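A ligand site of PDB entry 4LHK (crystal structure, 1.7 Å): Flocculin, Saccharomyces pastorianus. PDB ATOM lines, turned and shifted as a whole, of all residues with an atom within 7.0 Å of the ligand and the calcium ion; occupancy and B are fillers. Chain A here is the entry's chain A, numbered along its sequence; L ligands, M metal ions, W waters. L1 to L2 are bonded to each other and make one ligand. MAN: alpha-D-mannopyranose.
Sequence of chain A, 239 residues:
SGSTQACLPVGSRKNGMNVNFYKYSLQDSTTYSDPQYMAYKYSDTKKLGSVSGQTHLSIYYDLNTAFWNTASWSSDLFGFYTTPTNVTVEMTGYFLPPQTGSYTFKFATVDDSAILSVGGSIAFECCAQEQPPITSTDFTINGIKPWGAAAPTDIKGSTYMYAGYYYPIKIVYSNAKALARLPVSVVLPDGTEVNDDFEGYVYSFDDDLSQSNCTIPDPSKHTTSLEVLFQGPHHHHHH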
ATOM      1  N   SER A  29     -18.671   8.475  12.593  1.00  0.00           N
ATOM      2  CA  SER A  29     -19.764   8.043  11.742  1.00  0.00           C
ATOM      3  C   SER A  29     -21.126   8.570  12.192  1.00  0.00           C
ATOM      4  O   SER A  29     -22.198   8.176  11.678  1.00  0.00           O
ATOM      5  CB  SER A  29     -19.745   6.528  11.636  1.00  0.00           C
ATOM      6  OG  SER A  29     -19.878   6.001  12.932  1.00  0.00           O
ATOM      7  N   TYR A  32     -21.425  13.804  11.116  1.00  0.00           N
ATOM      8  CA  TYR A  32     -21.671  14.308   9.732  1.00  0.00           C
ATOM      9  C   TYR A  32     -23.176  14.258   9.329  1.00  0.00           C
ATOM     10  O   TYR A  32     -23.599  14.970   8.429  1.00  0.00           O
ATOM     11  CB  TYR A  32     -20.820  13.500   8.740  1.00  0.00           C
ATOM     12  CG  TYR A  32     -21.395  12.189   8.360  1.00  0.00           C
ATOM     13  CD1 TYR A  32     -21.387  11.112   9.237  1.00  0.00           C
ATOM     14  CD2 TYR A  32     -21.978  11.984   7.093  1.00  0.00           C
ATOM     15  CE1 TYR A  32     -21.918   9.899   8.871  1.00  0.00           C
ATOM     16  CE2 TYR A  32     -22.523  10.756   6.747  1.00  0.00           C
ATOM     17  CZ  TYR A  32     -22.504   9.744   7.619  1.00  0.00           C
ATOM     18  OH  TYR A  32     -23.032   8.530   7.276  1.00  0.00           O
ATOM     19  N   TRP A  68      -7.195   4.510   3.331  1.00  0.00           N
ATOM     20  CA  TRP A  68      -8.531   4.985   3.656  1.00  0.00           C
ATOM     21  C   TRP A  68      -8.932   5.033   5.126  1.00  0.00           C
ATOM     22  O   TRP A  68      -9.861   5.783   5.441  1.00  0.00           O
ATOM     23  CB  TRP A  68      -9.573   4.139   2.870  1.00  0.00           C
ATOM     24  CG  TRP A  68      -9.674   4.514   1.488  1.00  0.00           C
ATOM     25  CD1 TRP A  68      -8.831   5.331   0.747  1.00  0.00           C
ATOM     26  CD2 TRP A  68     -10.724   4.102   0.602  1.00  0.00           C
ATOM     27  NE1 TRP A  68      -9.312   5.426  -0.566  1.00  0.00           N
ATOM     28  CE2 TRP A  68     -10.457   4.682  -0.665  1.00  0.00           C
ATOM     29  CE3 TRP A  68     -11.842   3.279   0.755  1.00  0.00           C
ATOM     30  CZ2 TRP A  68     -11.352   4.470  -1.811  1.00  0.00           C
ATOM     31  CZ3 TRP A  68     -12.699   3.054  -0.372  1.00  0.00           C
ATOM     32  CH2 TRP A  68     -12.453   3.674  -1.614  1.00  0.00           C
ATOM     33  N   ASN A  69      -8.262   4.299   6.009  1.00  0.00           N
ATOM     34  CA  ASN A  69      -8.549   4.382   7.469  1.00  0.00           C
ATOM     35  C   ASN A  69      -7.669   5.412   8.147  1.00  0.00           C
ATOM     36  O   ASN A  69      -7.567   5.420   9.355  1.00  0.00           O
ATOM     37  CB  ASN A  69      -8.427   3.000   8.105  1.00  0.00           C
ATOM     38  CG  ASN A  69      -9.391   2.017   7.472  1.00  0.00           C
ATOM     39  OD1 ASN A  69     -10.507   2.377   7.085  1.00  0.00           O
ATOM     40  ND2 ASN A  69      -8.973   0.774   7.357  1.00  0.00           N
ATOM     41  N   PRO A  84      -7.800  16.508   4.115  1.00  0.00           N
ATOM     42  CA  PRO A  84      -9.112  16.514   3.495  1.00  0.00           C
ATOM     43  C   PRO A  84      -9.870  15.208   3.645  1.00  0.00           C
ATOM     44  O   PRO A  84     -11.013  15.114   3.255  1.00  0.00           O
ATOM     45  CB  PRO A  84      -8.804  16.798   2.022  1.00  0.00           C
ATOM     46  CG  PRO A  84      -7.383  16.531   1.826  1.00  0.00           C
ATOM     47  CD  PRO A  84      -6.744  16.843   3.156  1.00  0.00           C
ATOM     48  N   THR A  85      -9.183  14.209   4.173  1.00  0.00           N
ATOM     49  CA  THR A  85      -9.778  12.944   4.613  1.00  0.00           C
ATOM     50  C   THR A  85     -10.816  13.170   5.713  1.00  0.00           C
ATOM     51  O   THR A  85     -11.765  12.351   5.894  1.00  0.00           O
ATOM     52  CB  THR A  85      -8.687  12.007   5.173  1.00  0.00           C
ATOM     53  OG1 THR A  85      -7.831  12.792   6.021  1.00  0.00           O
ATOM     54  CG2 THR A  85      -7.860  11.354   4.001  1.00  0.00           C
ATOM     55  N   ASP A 111     -20.239  12.537  -0.673  1.00  0.00           N
ATOM     56  CA  ASP A 111     -19.459  11.675   0.175  1.00  0.00           C
ATOM     57  C   ASP A 111     -18.629  12.615   1.028  1.00  0.00           C
ATOM     58  O   ASP A 111     -17.661  13.190   0.478  1.00  0.00           O
ATOM     59  CB  ASP A 111     -18.573  10.706  -0.643  1.00  0.00           C
ATOM     60  CG  ASP A 111     -17.717   9.776   0.233  1.00  0.00           C
ATOM     61  OD1 ASP A 111     -17.538  10.137   1.416  1.00  0.00           O
ATOM     62  OD2 ASP A 111     -17.227   8.718  -0.277  1.00  0.00           O
ATOM     63  N   ASP A 112     -18.993  12.886   2.291  1.00  0.00           N
ATOM     64  CA  ASP A 112     -19.976  12.111   3.124  1.00  0.00           C
ATOM     65  C   ASP A 112     -21.333  12.794   3.364  1.00  0.00           C
ATOM     66  O   ASP A 112     -22.353  12.095   3.406  1.00  0.00           O
ATOM     67  CB  ASP A 112     -19.335  11.745   4.466  1.00  0.00           C
ATOM     68  CG  ASP A 112     -18.360  10.660   4.325  1.00  0.00           C
ATOM     69  OD1 ASP A 112     -18.771   9.476   4.312  1.00  0.00           O
ATOM     70  OD2 ASP A 112     -17.149  10.989   4.312  1.00  0.00           O
ATOM     71  N   LYS A 145     -24.483  10.486   2.727  1.00  0.00           N
ATOM     72  CA  LYS A 145     -24.052   9.151   2.344  1.00  0.00           C
ATOM     73  C   LYS A 145     -24.183   8.222   3.561  1.00  0.00           C
ATOM     74  O   LYS A 145     -23.591   8.504   4.634  1.00  0.00           O
ATOM     75  CB  LYS A 145     -22.608   9.162   1.858  1.00  0.00           C
ATOM     76  CG  LYS A 145     -22.107   7.790   1.428  1.00  0.00           C
ATOM     77  CD  LYS A 145     -20.639   7.867   1.084  1.00  0.00           C
ATOM     78  CE  LYS A 145     -20.126   6.552   0.518  1.00  0.00           C
ATOM     79  NZ  LYS A 145     -20.369   5.350   1.338  1.00  0.00           N
ATOM     80  N   PRO A 146     -24.966   7.146   3.420  1.00  0.00           N
ATOM     81  CA  PRO A 146     -25.056   6.186   4.543  1.00  0.00           C
ATOM     82  C   PRO A 146     -23.687   5.612   4.779  1.00  0.00           C
ATOM     83  O   PRO A 146     -22.909   5.388   3.826  1.00  0.00           O
ATOM     84  CB  PRO A 146     -25.961   5.110   3.996  1.00  0.00           C
ATOM     85  CG  PRO A 146     -26.743   5.768   2.907  1.00  0.00           C
ATOM     86  CD  PRO A 146     -25.830   6.765   2.274  1.00  0.00           C
ATOM     87  N   TRP A 147     -23.398   5.297   6.018  1.00  0.00           N
ATOM     88  CA  TRP A 147     -22.089   4.815   6.374  1.00  0.00           C
ATOM     89  C   TRP A 147     -21.794   3.461   5.717  1.00  0.00           C
ATOM     90  O   TRP A 147     -22.451   2.450   6.014  1.00  0.00           O
ATOM     91  CB  TRP A 147     -21.916   4.760   7.911  1.00  0.00           C
ATOM     92  CG  TRP A 147     -20.504   4.624   8.267  1.00  0.00           C
ATOM     93  CD1 TRP A 147     -19.836   3.481   8.565  1.00  0.00           C
ATOM     94  CD2 TRP A 147     -19.565   5.670   8.283  1.00  0.00           C
ATOM     95  NE1 TRP A 147     -18.520   3.751   8.806  1.00  0.00           N
ATOM     96  CE2 TRP A 147     -18.327   5.110   8.641  1.00  0.00           C
ATOM     97  CE3 TRP A 147     -19.659   7.059   8.080  1.00  0.00           C
ATOM     98  CZ2 TRP A 147     -17.156   5.880   8.770  1.00  0.00           C
ATOM     99  CZ3 TRP A 147     -18.462   7.834   8.171  1.00  0.00           C
ATOM    100  CH2 TRP A 147     -17.250   7.229   8.535  1.00  0.00           C
ATOM    101  N   GLY A 148     -20.799   3.441   4.835  1.00  0.00           N
ATOM    102  CA  GLY A 148     -20.393   2.259   4.133  1.00  0.00           C
ATOM    103  C   GLY A 148     -21.262   1.764   2.999  1.00  0.00           C
ATOM    104  O   GLY A 148     -21.073   0.640   2.531  1.00  0.00           O
ATOM    105  N   ALA A 149     -22.233   2.554   2.564  1.00  0.00           N
ATOM    106  CA  ALA A 149     -23.103   2.179   1.468  1.00  0.00           C
ATOM    107  C   ALA A 149     -23.293   3.340   0.507  1.00  0.00           C
ATOM    108  O   ALA A 149     -22.937   4.505   0.754  1.00  0.00           O
ATOM    109  CB  ALA A 149     -24.457   1.717   1.978  1.00  0.00           C
ATOM    110  N   ALA A 150     -23.880   2.987  -0.627  1.00  0.00           N
ATOM    111  CA  ALA A 150     -24.065   3.926  -1.713  1.00  0.00           C
ATOM    112  C   ALA A 150     -24.790   5.202  -1.297  1.00  0.00           C
ATOM    113  O   ALA A 150     -25.789   5.186  -0.582  1.00  0.00           O
ATOM    114  CB  ALA A 150     -24.780   3.265  -2.879  1.00  0.00           C
ATOM    115  N   ALA A 151     -24.255   6.310  -1.779  1.00  0.00           N
ATOM    116  CA  ALA A 151     -24.862   7.605  -1.613  1.00  0.00           C
ATOM    117  C   ALA A 151     -26.014   7.790  -2.619  1.00  0.00           C
ATOM    118  O   ALA A 151     -25.931   7.278  -3.750  1.00  0.00           O
ATOM    119  CB  ALA A 151     -23.793   8.668  -1.816  1.00  0.00           C
ATOM    120  N   TYR A 173     -20.203  21.123   3.771  1.00  0.00           N
ATOM    121  CA  TYR A 173     -19.792  19.820   3.282  1.00  0.00           C
ATOM    122  C   TYR A 173     -18.888  19.122   4.310  1.00  0.00           C
ATOM    123  O   TYR A 173     -18.014  19.799   4.880  1.00  0.00           O
ATOM    124  CB  TYR A 173     -19.031  19.962   1.910  1.00  0.00           C
ATOM    125  CG  TYR A 173     -18.319  18.671   1.639  1.00  0.00           C
ATOM    126  CD1 TYR A 173     -18.981  17.597   1.113  1.00  0.00           C
ATOM    127  CD2 TYR A 173     -16.966  18.513   1.964  1.00  0.00           C
ATOM    128  CE1 TYR A 173     -18.365  16.379   0.961  1.00  0.00           C
ATOM    129  CE2 TYR A 173     -16.331  17.313   1.851  1.00  0.00           C
ATOM    130  CZ  TYR A 173     -17.026  16.244   1.324  1.00  0.00           C
ATOM    131  OH  TYR A 173     -16.348  15.080   1.229  1.00  0.00           O
ATOM    132  N   SER A 174     -19.073  17.828   4.551  1.00  0.00           N
ATOM    133  CA  SER A 174     -18.187  17.080   5.453  1.00  0.00           C
ATOM    134  C   SER A 174     -17.661  15.812   4.851  1.00  0.00           C
ATOM    135  O   SER A 174     -18.415  15.038   4.236  1.00  0.00           O
ATOM    136  CB  SER A 174     -18.918  16.720   6.766  1.00  0.00           C
ATOM    137  OG  SER A 174     -19.199  17.892   7.419  1.00  0.00           O
ATOM    138  N   ASN A 175     -16.360  15.558   5.095  1.00  0.00           N
ATOM    139  CA  ASN A 175     -15.720  14.293   4.809  1.00  0.00           C
ATOM    140  C   ASN A 175     -15.314  13.688   6.112  1.00  0.00           C
ATOM    141  O   ASN A 175     -14.710  14.360   6.921  1.00  0.00           O
ATOM    142  CB  ASN A 175     -14.500  14.418   3.898  1.00  0.00           C
ATOM    143  CG  ASN A 175     -14.045  13.057   3.346  1.00  0.00           C
ATOM    144  OD1 ASN A 175     -14.753  12.106   3.411  1.00  0.00           O
ATOM    145  ND2 ASN A 175     -12.856  12.996   2.831  1.00  0.00           N
ATOM    146  N   ALA A 176     -15.740  12.456   6.342  1.00  0.00           N
ATOM    147  CA  ALA A 176     -15.496  11.748   7.588  1.00  0.00           C
ATOM    148  C   ALA A 176     -14.311  10.818   7.496  1.00  0.00           C
ATOM    149  O   ALA A 176     -13.676  10.503   8.498  1.00  0.00           O
ATOM    150  CB  ALA A 176     -16.752  10.995   7.949  1.00  0.00           C
ATOM    151  N   LYS A 177     -14.011  10.390   6.273  1.00  0.00           N
ATOM    152  CA  LYS A 177     -12.872   9.574   5.962  1.00  0.00           C
ATOM    153  C   LYS A 177     -12.689   9.371   4.458  1.00  0.00           C
ATOM    154  O   LYS A 177     -13.668   9.448   3.698  1.00  0.00           O
ATOM    155  CB  LYS A 177     -12.887   8.163   6.607  1.00  0.00           C
ATOM    156  CG  LYS A 177     -13.952   7.246   6.124  1.00  0.00           C
ATOM    157  CD  LYS A 177     -13.975   5.934   6.902  1.00  0.00           C
ATOM    158  CE  LYS A 177     -12.760   5.055   6.632  1.00  0.00           C
ATOM    159  NZ  LYS A 177     -12.891   3.716   7.286  1.00  0.00           N
ATOM    160  N   ALA A 178     -11.450   9.119   4.051  1.00  0.00           N
ATOM    161  CA  ALA A 178     -11.143   8.666   2.710  1.00  0.00           C
ATOM    162  C   ALA A 178     -11.598   9.729   1.617  1.00  0.00           C
ATOM    163  O   ALA A 178     -11.258  10.933   1.727  1.00  0.00           O
ATOM    164  CB  ALA A 178     -11.684   7.264   2.504  1.00  0.00           C
ATOM    165  N   LEU A 179     -12.398   9.303   0.661  1.00  0.00           N
ATOM    166  CA  LEU A 179     -12.727  10.099  -0.530  1.00  0.00           C
ATOM    167  C   LEU A 179     -13.649  11.226  -0.129  1.00  0.00           C
ATOM    168  O   LEU A 179     -14.519  11.071   0.724  1.00  0.00           O
ATOM    169  CB  LEU A 179     -13.510   9.231  -1.531  1.00  0.00           C
ATOM    170  CG  LEU A 179     -13.026   7.911  -1.977  1.00  0.00           C
ATOM    171  CD1 LEU A 179     -13.879   7.386  -3.154  1.00  0.00           C
ATOM    172  CD2 LEU A 179     -11.567   8.084  -2.327  1.00  0.00           C
ATOM    173  N   ALA A 180     -13.431  12.366  -0.744  1.00  0.00           N
ATOM    174  CA  ALA A 180     -14.396  13.478  -0.730  1.00  0.00           C
ATOM    175  C   ALA A 180     -15.019  13.699  -2.138  1.00  0.00           C
ATOM    176  O   ALA A 180     -14.310  13.817  -3.142  1.00  0.00           O
ATOM    177  CB  ALA A 180     -13.698  14.733  -0.236  1.00  0.00           C
ATOM    178  N   ARG A 181     -16.335  13.789  -2.185  1.00  0.00           N
ATOM    179  CA  ARG A 181     -17.032  13.994  -3.434  1.00  0.00           C
ATOM    180  C   ARG A 181     -18.231  14.937  -3.228  1.00  0.00           C
ATOM    181  O   ARG A 181     -19.106  14.663  -2.376  1.00  0.00           O
ATOM    182  CB  ARG A 181     -17.655  12.706  -4.021  1.00  0.00           C
ATOM    183  CG  ARG A 181     -16.814  11.618  -4.589  1.00  0.00           C
ATOM    184  CD  ARG A 181     -17.732  10.639  -5.394  1.00  0.00           C
ATOM    185  NE  ARG A 181     -18.165  11.111  -6.745  1.00  0.00           N
ATOM    186  CZ  ARG A 181     -18.679  10.313  -7.686  1.00  0.00           C
ATOM    187  NH1 ARG A 181     -18.878   9.021  -7.475  1.00  0.00           N
ATOM    188  NH2 ARG A 181     -19.028  10.824  -8.902  1.00  0.00           N
HETATM  189  C1  MAN L   1     -15.712   4.391   2.606  1.00  0.00           C
HETATM  190  C2  MAN L   1     -15.393   5.523   1.594  1.00  0.00           C
HETATM  191  C3  MAN L   1     -15.479   6.860   2.293  1.00  0.00           C
HETATM  192  C4  MAN L   1     -16.788   7.013   3.069  1.00  0.00           C
HETATM  193  C5  MAN L   1     -17.038   5.836   4.006  1.00  0.00           C
HETATM  194  C6  MAN L   1     -18.313   5.877   4.889  1.00  0.00           C
HETATM  195  O1  MAN L   1     -14.567   4.282   3.457  1.00  0.00           O
HETATM  196  O2  MAN L   1     -16.263   5.563   0.535  1.00  0.00           O
HETATM  197  O3  MAN L   1     -15.289   7.934   1.387  1.00  0.00           O
HETATM  198  O4  MAN L   1     -16.697   8.188   3.779  1.00  0.00           O
HETATM  199  O5  MAN L   1     -16.984   4.618   3.249  1.00  0.00           O
HETATM  200  O6  MAN L   1     -19.463   5.872   4.051  1.00  0.00           O
HETATM  201  C1  MAN L   2     -15.853   4.508  -0.367  1.00  0.00           C
HETATM  202  C2  MAN L   2     -16.531   4.698  -1.685  1.00  0.00           C
HETATM  203  C3  MAN L   2     -18.044   4.606  -1.419  1.00  0.00           C
HETATM  204  C4  MAN L   2     -18.463   3.298  -0.700  1.00  0.00           C
HETATM  205  C5  MAN L   2     -17.526   3.052   0.502  1.00  0.00           C
HETATM  206  C6  MAN L   2     -17.675   1.682   1.201  1.00  0.00           C
HETATM  207  O2  MAN L   2     -16.074   3.604  -2.435  1.00  0.00           O
HETATM  208  O3  MAN L   2     -18.664   4.694  -2.677  1.00  0.00           O
HETATM  209  O4  MAN L   2     -19.801   3.286  -0.207  1.00  0.00           O
HETATM  210  O5  MAN L   2     -16.173   3.205   0.077  1.00  0.00           O
HETATM  211  O6  MAN L   2     -17.553   0.659   0.238  1.00  0.00           O
HETATM  212 CA    CA M   1     -15.541  10.140   2.637  1.00  0.00          CA
HETATM  213  O   HOH W   1     -18.473   7.689  -2.484  1.00  0.00           O
HETATM  214  O   HOH W   2     -15.561   1.107  -2.336  1.00  0.00           O
HETATM  215  O   HOH W   3     -20.847   7.881   4.912  1.00  0.00           O
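O3 of MAN L1 sits close to N of Leu 179 (3.3 Å).
An oxygen (O4) of MAN L2 is in hydrogen-bond range of the side-chain amino group (NZ) of Lys 145.
O6 of MAN L1 sits at hydrogen-bond distance from N of Gly 148.
The backbone carbonyl oxygen of Pro 146 is in hydrogen-bond range of an oxygen (O6) of MAN L1 (3.5 Å).
The backbone carbonyl oxygen of Ala 149 is in hydrogen-bond range of an oxygen (O4) of MAN L2 (3.5 Å).
The side-chain amide nitrogen of Asn 175 lies within hydrogen-bond range of the backbone carbonyl oxygen of Ala 178.
ND2 of Asn 175 is in hydrogen-bond range of O of Thr 85, 3.3 Å away.
The backbone NH (N) of Lys 177 sits close to the backbone carbonyl oxygen (O) of Thr 85.
NZ of Lys 177 lies within hydrogen-bond range of OD1 of Asn 69, 2.7 Å away.
The backbone NH (N) of Asp 111 lies within hydrogen-bond range of the backbone carbonyl oxygen (O) of Arg 181 (3.0 Å).
The side-chain carboxylate of Asp 112 sits close to the backbone NH of Ala 176 (2.9 Å).
N of Asp 112 sits at hydrogen-bond distance from O of Ser 174 (3.0 Å).
The side-chain hydroxyl (OH) of Tyr 32 sits at hydrogen-bond distance from the backbone carbonyl oxygen (O) of Lys 145 (2.7 Å).
Merely in contact with the ligand: Trp 68, Trp 147 and Ala 178.
Five residues have an atom within 4 Å of the calcium ion: Asp 111, Asp 112, Asn 175, Lys 177 and Leu 179.
The nearest printed residue that does not touch the calcium ion is Ala 178 (4.1 Å).
OD1 of Asn 175 is bound to the calcium ion, 2.3 Å away.
O of Lys 177 is bound to the calcium ion (2.3 Å).
OD1 of Asp 111 is bound to the calcium ion, 2.3 Å away.
The calcium ion is bound by the backbone carbonyl oxygen (O) of Leu 179 (2.4 Å).
The calcium ion is bound by OD2 of Asp 112 (2.5 Å).
An oxygen (O4) of MAN L1 binds the calcium ion (2.5 Å).
O3 of MAN L1 binds the calcium ion (2.5 Å).
The calcium ion has seven donor atoms within binding distance.
Water W1 lies within hydrogen-bond range of OD2 of Asp 111 (2.7 Å) and O3 of MAN L2 (3.0 Å).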
